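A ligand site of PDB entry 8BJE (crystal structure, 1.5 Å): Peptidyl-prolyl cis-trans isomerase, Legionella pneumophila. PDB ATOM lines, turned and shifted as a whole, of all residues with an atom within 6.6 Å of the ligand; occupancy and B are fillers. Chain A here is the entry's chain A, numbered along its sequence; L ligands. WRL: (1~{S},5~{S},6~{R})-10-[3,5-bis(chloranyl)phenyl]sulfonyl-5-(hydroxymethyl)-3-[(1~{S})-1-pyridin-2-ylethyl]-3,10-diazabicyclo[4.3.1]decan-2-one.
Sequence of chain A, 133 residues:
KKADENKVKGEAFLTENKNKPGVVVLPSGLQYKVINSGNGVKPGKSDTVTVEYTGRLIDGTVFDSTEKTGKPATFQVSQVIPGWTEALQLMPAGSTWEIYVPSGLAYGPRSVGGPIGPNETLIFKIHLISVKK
An oxygen (O3) of the ligand is in hydrogen-bond range of the backbone NH of Ile 81, at 3.0 Å. N3 of the ligand is in hydrogen-bond range of OH of Tyr 107, 2.7 Å away.
Tyr 53 touches the ligand. CE1 of Phe 63 touches O1 of the ligand, at 3.4 Å. Asp 64 touches the ligand. Phe 75 touches the ligand (CZ to C7, 3.6 Å). Val 80 touches the ligand. Trp 84 touches the ligand. NH1 of Arg 110 touches CL2 of the ligand (3.3 Å). Ile 116 touches the ligand (CG1 to CL2, 3.9 Å). Phe 124 touches the ligand (CE2 to O1, 3.3 Å). Hydrophobic or aromatic side chains within 4 Å of the ligand: Tyr 53, Phe 63, Phe 75, Val 80, Ile 81, Trp 84, Tyr 107, Ile 116 and Phe 124. 11 residues have an atom within 4 Å of the ligand: Tyr 53, Phe 63, Asp 64, Phe 75, Val 80, Ile 81, Trp 84, Tyr 107, Arg 110, Ile 116 and Phe 124. The nearest printed residue that does not touch the ligand is Gln 79 (4.1 Å).
The backbone NH of Gly 55 sits at hydrogen-bond distance from the backbone carbonyl oxygen of Asp 64, at 2.8 Å. The guanidinium group (NE) of Arg 110 sits close to the backbone carbonyl oxygen (O) of Ile 116 (3.4 Å). The side-chain hydroxyl (OH) of Tyr 53 lies within hydrogen-bond range of the side-chain carboxylate (OD2) of Asp 64 (2.7 Å). The backbone NH (N) of Phe 63 is in hydrogen-bond range of the backbone carbonyl oxygen (O) of Gly 55 (2.9 Å).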
ATOM      1  N   TYR A  53      21.019  14.452 -27.476  1.00  0.00           N
ATOM      2  CA  TYR A  53      20.630  13.507 -26.409  1.00  0.00           C
ATOM      3  C   TYR A  53      21.732  12.519 -26.099  1.00  0.00           C
ATOM      4  O   TYR A  53      22.639  12.361 -26.903  1.00  0.00           O
ATOM      5  CB  TYR A  53      19.366  12.733 -26.769  1.00  0.00           C
ATOM      6  CG  TYR A  53      19.549  11.677 -27.816  1.00  0.00           C
ATOM      7  CD1 TYR A  53      19.462  11.998 -29.155  1.00  0.00           C
ATOM      8  CD2 TYR A  53      19.778  10.360 -27.468  1.00  0.00           C
ATOM      9  CE1 TYR A  53      19.622  11.038 -30.125  1.00  0.00           C
ATOM     10  CE2 TYR A  53      19.944   9.381 -28.429  1.00  0.00           C
ATOM     11  CZ  TYR A  53      19.867   9.730 -29.768  1.00  0.00           C
ATOM     12  OH  TYR A  53      20.013   8.830 -30.766  1.00  0.00           O
ATOM     13  N   THR A  54      21.655  11.965 -24.916  1.00  0.00           N
ATOM     14  CA  THR A  54      22.578  10.908 -24.469  1.00  0.00           C
ATOM     15  C   THR A  54      21.674   9.909 -23.757  1.00  0.00           C
ATOM     16  O   THR A  54      20.839  10.372 -23.001  1.00  0.00           O
ATOM     17  CB  THR A  54      23.678  11.454 -23.567  1.00  0.00           C
ATOM     18  OG1 THR A  54      24.485  12.357 -24.310  1.00  0.00           O
ATOM     19  CG2 THR A  54      24.540  10.351 -23.003  1.00  0.00           C
ATOM     20  N   GLY A  55      21.801   8.625 -24.042  1.00  0.00           N
ATOM     21  CA  GLY A  55      21.057   7.539 -23.383  1.00  0.00           C
ATOM     22  C   GLY A  55      22.030   6.741 -22.558  1.00  0.00           C
ATOM     23  O   GLY A  55      23.119   6.484 -23.050  1.00  0.00           O
ATOM     24  N   PHE A  63      24.959   4.379 -23.909  1.00  0.00           N
ATOM     25  CA  PHE A  63      24.749   3.427 -25.022  1.00  0.00           C
ATOM     26  C   PHE A  63      24.421   4.176 -26.311  1.00  0.00           C
ATOM     27  O   PHE A  63      24.315   3.545 -27.329  1.00  0.00           O
ATOM     28  CB  PHE A  63      23.654   2.414 -24.678  1.00  0.00           C
ATOM     29  CG  PHE A  63      22.301   2.982 -24.348  1.00  0.00           C
ATOM     30  CD1 PHE A  63      21.425   3.353 -25.349  1.00  0.00           C
ATOM     31  CD2 PHE A  63      21.903   3.123 -23.034  1.00  0.00           C
ATOM     32  CE1 PHE A  63      20.173   3.876 -25.037  1.00  0.00           C
ATOM     33  CE2 PHE A  63      20.657   3.640 -22.727  1.00  0.00           C
ATOM     34  CZ  PHE A  63      19.803   4.014 -23.723  1.00  0.00           C
ATOM     35  N   ASP A  64      24.174   5.482 -26.227  1.00  0.00           N
ATOM     36  CA  ASP A  64      23.883   6.294 -27.424  1.00  0.00           C
ATOM     37  C   ASP A  64      24.072   7.780 -27.093  1.00  0.00           C
ATOM     38  O   ASP A  64      23.827   8.143 -25.967  1.00  0.00           O
ATOM     39  CB  ASP A  64      22.490   6.005 -27.959  1.00  0.00           C
ATOM     40  CG  ASP A  64      22.312   6.407 -29.411  1.00  0.00           C
ATOM     41  OD1 ASP A  64      23.320   6.548 -30.058  1.00  0.00           O
ATOM     42  OD2 ASP A  64      21.181   6.570 -29.847  1.00  0.00           O
ATOM     43  N   PHE A  75      13.659  13.408 -35.069  1.00  0.00           N
ATOM     44  CA  PHE A  75      12.696  12.315 -34.843  1.00  0.00           C
ATOM     45  C   PHE A  75      11.249  12.790 -34.987  1.00  0.00           C
ATOM     46  O   PHE A  75      10.984  13.928 -34.606  1.00  0.00           O
ATOM     47  CB  PHE A  75      12.854  11.799 -33.404  1.00  0.00           C
ATOM     48  CG  PHE A  75      14.206  11.234 -33.053  1.00  0.00           C
ATOM     49  CD1 PHE A  75      14.593   9.986 -33.511  1.00  0.00           C
ATOM     50  CD2 PHE A  75      15.082  11.939 -32.244  1.00  0.00           C
ATOM     51  CE1 PHE A  75      15.829   9.460 -33.174  1.00  0.00           C
ATOM     52  CE2 PHE A  75      16.319  11.420 -31.915  1.00  0.00           C
ATOM     53  CZ  PHE A  75      16.693  10.188 -32.387  1.00  0.00           C
ATOM     54  N   GLN A  79       7.001   8.311 -33.240  1.00  0.00           N
ATOM     55  CA  GLN A  79       7.713   7.109 -33.758  1.00  0.00           C
ATOM     56  C   GLN A  79       8.955   6.773 -32.935  1.00  0.00           C
ATOM     57  O   GLN A  79       9.813   6.072 -33.459  1.00  0.00           O
ATOM     58  CB  GLN A  79       7.992   7.411 -35.230  1.00  0.00           C
ATOM     59  CG  GLN A  79       6.748   7.318 -36.089  1.00  0.00           C
ATOM     60  CD  GLN A  79       7.025   7.770 -37.501  1.00  0.00           C
ATOM     61  OE1 GLN A  79       8.140   8.128 -37.845  1.00  0.00           O
ATOM     62  NE2 GLN A  79       5.990   7.751 -38.322  1.00  0.00           N
ATOM     63  N   VAL A  80       9.060   7.254 -31.701  1.00  0.00           N
ATOM     64  CA  VAL A  80      10.156   6.882 -30.760  1.00  0.00           C
ATOM     65  C   VAL A  80       9.493   6.142 -29.582  1.00  0.00           C
ATOM     66  O   VAL A  80       8.281   5.958 -29.608  1.00  0.00           O
ATOM     67  CB  VAL A  80      10.975   8.089 -30.297  1.00  0.00           C
ATOM     68  CG1 VAL A  80      11.927   8.567 -31.376  1.00  0.00           C
ATOM     69  CG2 VAL A  80      10.099   9.234 -29.822  1.00  0.00           C
ATOM     70  N   ILE A  81      10.292   5.725 -28.605  1.00  0.00           N
ATOM     71  CA  ILE A  81       9.765   4.980 -27.431  1.00  0.00           C
ATOM     72  C   ILE A  81       8.691   5.831 -26.717  1.00  0.00           C
ATOM     73  O   ILE A  81       8.822   7.032 -26.707  1.00  0.00           O
ATOM     74  CB  ILE A  81      10.904   4.550 -26.486  1.00  0.00           C
ATOM     75  CG1 ILE A  81      11.841   5.676 -26.059  1.00  0.00           C
ATOM     76  CG2 ILE A  81      11.677   3.390 -27.097  1.00  0.00           C
ATOM     77  CD1 ILE A  81      12.792   5.269 -24.960  1.00  0.00           C
ATOM     78  N   PRO A  82       7.664   5.182 -26.115  1.00  0.00           N
ATOM     79  CA  PRO A  82       6.606   5.921 -25.409  1.00  0.00           C
ATOM     80  C   PRO A  82       7.132   6.965 -24.424  1.00  0.00           C
ATOM     81  O   PRO A  82       6.546   8.010 -24.362  1.00  0.00           O
ATOM     82  CB  PRO A  82       5.867   4.814 -24.659  1.00  0.00           C
ATOM     83  CG  PRO A  82       6.053   3.588 -25.521  1.00  0.00           C
ATOM     84  CD  PRO A  82       7.449   3.746 -26.095  1.00  0.00           C
ATOM     85  N   TRP A  84       9.802   8.805 -24.616  1.00  0.00           N
ATOM     86  CA  TRP A  84      10.188   9.998 -25.419  1.00  0.00           C
ATOM     87  C   TRP A  84       8.920  10.690 -25.932  1.00  0.00           C
ATOM     88  O   TRP A  84       8.846  11.891 -25.805  1.00  0.00           O
ATOM     89  CB  TRP A  84      11.125   9.582 -26.563  1.00  0.00           C
ATOM     90  CG  TRP A  84      12.571   9.619 -26.222  1.00  0.00           C
ATOM     91  CD1 TRP A  84      13.192   8.905 -25.243  1.00  0.00           C
ATOM     92  CD2 TRP A  84      13.601  10.413 -26.852  1.00  0.00           C
ATOM     93  NE1 TRP A  84      14.524   9.204 -25.219  1.00  0.00           N
ATOM     94  CE2 TRP A  84      14.804  10.118 -26.188  1.00  0.00           C
ATOM     95  CE3 TRP A  84      13.609  11.326 -27.907  1.00  0.00           C
ATOM     96  CZ2 TRP A  84      16.012  10.719 -26.540  1.00  0.00           C
ATOM     97  CZ3 TRP A  84      14.809  11.916 -28.257  1.00  0.00           C
ATOM     98  CH2 TRP A  84      15.983  11.617 -27.585  1.00  0.00           C
ATOM     99  N   ALA A 106       9.586   1.841 -22.681  1.00  0.00           N
ATOM    100  CA  ALA A 106      10.760   1.783 -23.583  1.00  0.00           C
ATOM    101  C   ALA A 106      10.658   0.522 -24.452  1.00  0.00           C
ATOM    102  O   ALA A 106       9.773   0.511 -25.292  1.00  0.00           O
ATOM    103  CB  ALA A 106      12.019   1.882 -22.772  1.00  0.00           C
ATOM    104  N   TYR A 107      11.485  -0.490 -24.223  1.00  0.00           N
ATOM    105  CA  TYR A 107      11.507  -1.723 -25.066  1.00  0.00           C
ATOM    106  C   TYR A 107      10.880  -2.901 -24.329  1.00  0.00           C
ATOM    107  O   TYR A 107      10.700  -3.935 -24.963  1.00  0.00           O
ATOM    108  CB  TYR A 107      12.939  -1.921 -25.533  1.00  0.00           C
ATOM    109  CG  TYR A 107      13.394  -0.795 -26.407  1.00  0.00           C
ATOM    110  CD1 TYR A 107      12.985  -0.721 -27.725  1.00  0.00           C
ATOM    111  CD2 TYR A 107      14.165   0.240 -25.904  1.00  0.00           C
ATOM    112  CE1 TYR A 107      13.362   0.334 -28.536  1.00  0.00           C
ATOM    113  CE2 TYR A 107      14.555   1.296 -26.698  1.00  0.00           C
ATOM    114  CZ  TYR A 107      14.150   1.341 -28.017  1.00  0.00           C
ATOM    115  OH  TYR A 107      14.525   2.385 -28.796  1.00  0.00           O
ATOM    116  N   ARG A 110      11.221  -7.518 -23.643  1.00  0.00           N
ATOM    117  CA  ARG A 110      12.283  -7.672 -24.677  1.00  0.00           C
ATOM    118  C   ARG A 110      13.086  -8.939 -24.457  1.00  0.00           C
ATOM    119  O   ARG A 110      14.288  -8.799 -24.210  1.00  0.00           O
ATOM    120  CB  ARG A 110      13.284  -6.517 -24.604  1.00  0.00           C
ATOM    121  CG  ARG A 110      13.716  -5.962 -25.957  1.00  0.00           C
ATOM    122  CD  ARG A 110      14.986  -5.132 -25.819  1.00  0.00           C
ATOM    123  NE  ARG A 110      15.566  -4.766 -27.101  1.00  0.00           N
ATOM    124  CZ  ARG A 110      15.147  -3.753 -27.855  1.00  0.00           C
ATOM    125  NH1 ARG A 110      15.772  -2.591 -27.830  1.00  0.00           N
ATOM    126  NH2 ARG A 110      14.096  -3.912 -28.632  1.00  0.00           N
ATOM    127  N   PRO A 115      22.182  -3.609 -26.860  1.00  0.00           N
ATOM    128  CA  PRO A 115      22.448  -2.412 -26.090  1.00  0.00           C
ATOM    129  C   PRO A 115      21.426  -2.463 -24.942  1.00  0.00           C
ATOM    130  O   PRO A 115      21.828  -2.287 -23.830  1.00  0.00           O
ATOM    131  CB  PRO A 115      22.282  -1.288 -27.114  1.00  0.00           C
ATOM    132  CG  PRO A 115      21.364  -1.851 -28.166  1.00  0.00           C
ATOM    133  CD  PRO A 115      21.735  -3.317 -28.224  1.00  0.00           C
ATOM    134  N   ILE A 116      20.164  -2.749 -25.254  1.00  0.00           N
ATOM    135  CA  ILE A 116      19.041  -2.740 -24.267  1.00  0.00           C
ATOM    136  C   ILE A 116      18.622  -4.173 -23.947  1.00  0.00           C
ATOM    137  O   ILE A 116      18.085  -4.841 -24.809  1.00  0.00           O
ATOM    138  CB  ILE A 116      17.866  -1.925 -24.848  1.00  0.00           C
ATOM    139  CG1 ILE A 116      18.309  -0.574 -25.424  1.00  0.00           C
ATOM    140  CG2 ILE A 116      16.763  -1.760 -23.822  1.00  0.00           C
ATOM    141  CD1 ILE A 116      19.110   0.272 -24.475  1.00  0.00           C
ATOM    142  N   LEU A 122      15.804   3.077 -18.716  1.00  0.00           N
ATOM    143  CA  LEU A 122      16.712   3.937 -19.518  1.00  0.00           C
ATOM    144  C   LEU A 122      16.691   5.378 -19.003  1.00  0.00           C
ATOM    145  O   LEU A 122      15.632   5.839 -18.633  1.00  0.00           O
ATOM    146  CB  LEU A 122      16.277   3.866 -20.978  1.00  0.00           C
ATOM    147  CG  LEU A 122      16.099   2.489 -21.606  1.00  0.00           C
ATOM    148  CD1 LEU A 122      15.654   2.635 -23.054  1.00  0.00           C
ATOM    149  CD2 LEU A 122      17.383   1.673 -21.528  1.00  0.00           C
ATOM    150  N   PHE A 124      17.743   9.282 -20.057  1.00  0.00           N
ATOM    151  CA  PHE A 124      18.105  10.131 -21.205  1.00  0.00           C
ATOM    152  C   PHE A 124      18.228  11.598 -20.857  1.00  0.00           C
ATOM    153  O   PHE A 124      17.369  12.102 -20.161  1.00  0.00           O
ATOM    154  CB  PHE A 124      17.066  10.037 -22.306  1.00  0.00           C
ATOM    155  CG  PHE A 124      16.861   8.674 -22.882  1.00  0.00           C
ATOM    156  CD1 PHE A 124      15.868   7.849 -22.389  1.00  0.00           C
ATOM    157  CD2 PHE A 124      17.610   8.235 -23.958  1.00  0.00           C
ATOM    158  CE1 PHE A 124      15.649   6.601 -22.940  1.00  0.00           C
ATOM    159  CE2 PHE A 124      17.384   6.993 -24.503  1.00  0.00           C
ATOM    160  CZ  PHE A 124      16.407   6.176 -24.000  1.00  0.00           C
HETATM  161  N1  WRL L   1      16.572   5.723 -28.787  1.00  0.00           N
HETATM  162  N3  WRL L   1      14.720   1.839 -31.421  1.00  0.00           N
HETATM  163  C4  WRL L   1      15.105   5.715 -28.686  1.00  0.00           C
HETATM  164  C5  WRL L   1      14.650   7.114 -28.313  1.00  0.00           C
HETATM  165  C6  WRL L   1      15.163   8.137 -29.334  1.00  0.00           C
HETATM  166  C7  WRL L   1      16.670   8.058 -29.444  1.00  0.00           C
HETATM  167  C8  WRL L   1      17.152   6.646 -29.786  1.00  0.00           C
HETATM  168  C10 WRL L   1      18.048   6.344 -32.144  1.00  0.00           C
HETATM  169  C13 WRL L   1      13.774   4.994 -33.181  1.00  0.00           C
HETATM  170  C15 WRL L   1      15.185   0.632 -31.749  1.00  0.00           C
HETATM  171  C17 WRL L   1      15.210   1.133 -34.043  1.00  0.00           C
HETATM  172  C20 WRL L   1      17.724   2.315 -28.579  1.00  0.00           C
HETATM  173  C21 WRL L   1      18.377   1.283 -29.234  1.00  0.00           C
HETATM  174  C22 WRL L   1      19.577   1.483 -29.886  1.00  0.00           C
HETATM  175  C1  WRL L   1      20.115   2.752 -29.879  1.00  0.00           C
HETATM  176  C11 WRL L   1      16.300   4.773 -31.251  1.00  0.00           C
HETATM  177  C12 WRL L   1      13.988   4.078 -31.980  1.00  0.00           C
HETATM  178  C14 WRL L   1      14.503   2.711 -32.414  1.00  0.00           C
HETATM  179  C16 WRL L   1      15.431   0.234 -33.033  1.00  0.00           C
HETATM  180  C18 WRL L   1      14.738   2.396 -33.732  1.00  0.00           C
HETATM  181  C19 WRL L   1      14.262   5.190 -29.848  1.00  0.00           C
HETATM  182  C2  WRL L   1      19.499   3.799 -29.234  1.00  0.00           C
HETATM  183  C3  WRL L   1      18.289   3.577 -28.589  1.00  0.00           C
HETATM  184  C9  WRL L   1      16.850   6.198 -31.232  1.00  0.00           C
HETATM  185  N2  WRL L   1      14.864   4.710 -30.964  1.00  0.00           N
HETATM  186  O1  WRL L   1      18.516   5.778 -27.308  1.00  0.00           O
HETATM  187  O2  WRL L   1      17.628   6.267 -33.498  1.00  0.00           O
HETATM  188  O3  WRL L   1      13.048   5.216 -29.743  1.00  0.00           O
HETATM  189  O4  WRL L   1      16.607   4.320 -26.795  1.00  0.00           O
HETATM  190  S1  WRL L   1      17.488   4.906 -27.751  1.00  0.00           S
HETATM  191 CL1  WRL L   1      21.616   3.037 -30.709  1.00  0.00          CL
HETATM  192 CL2  WRL L   1      17.660  -0.296 -29.224  1.00  0.00          CL
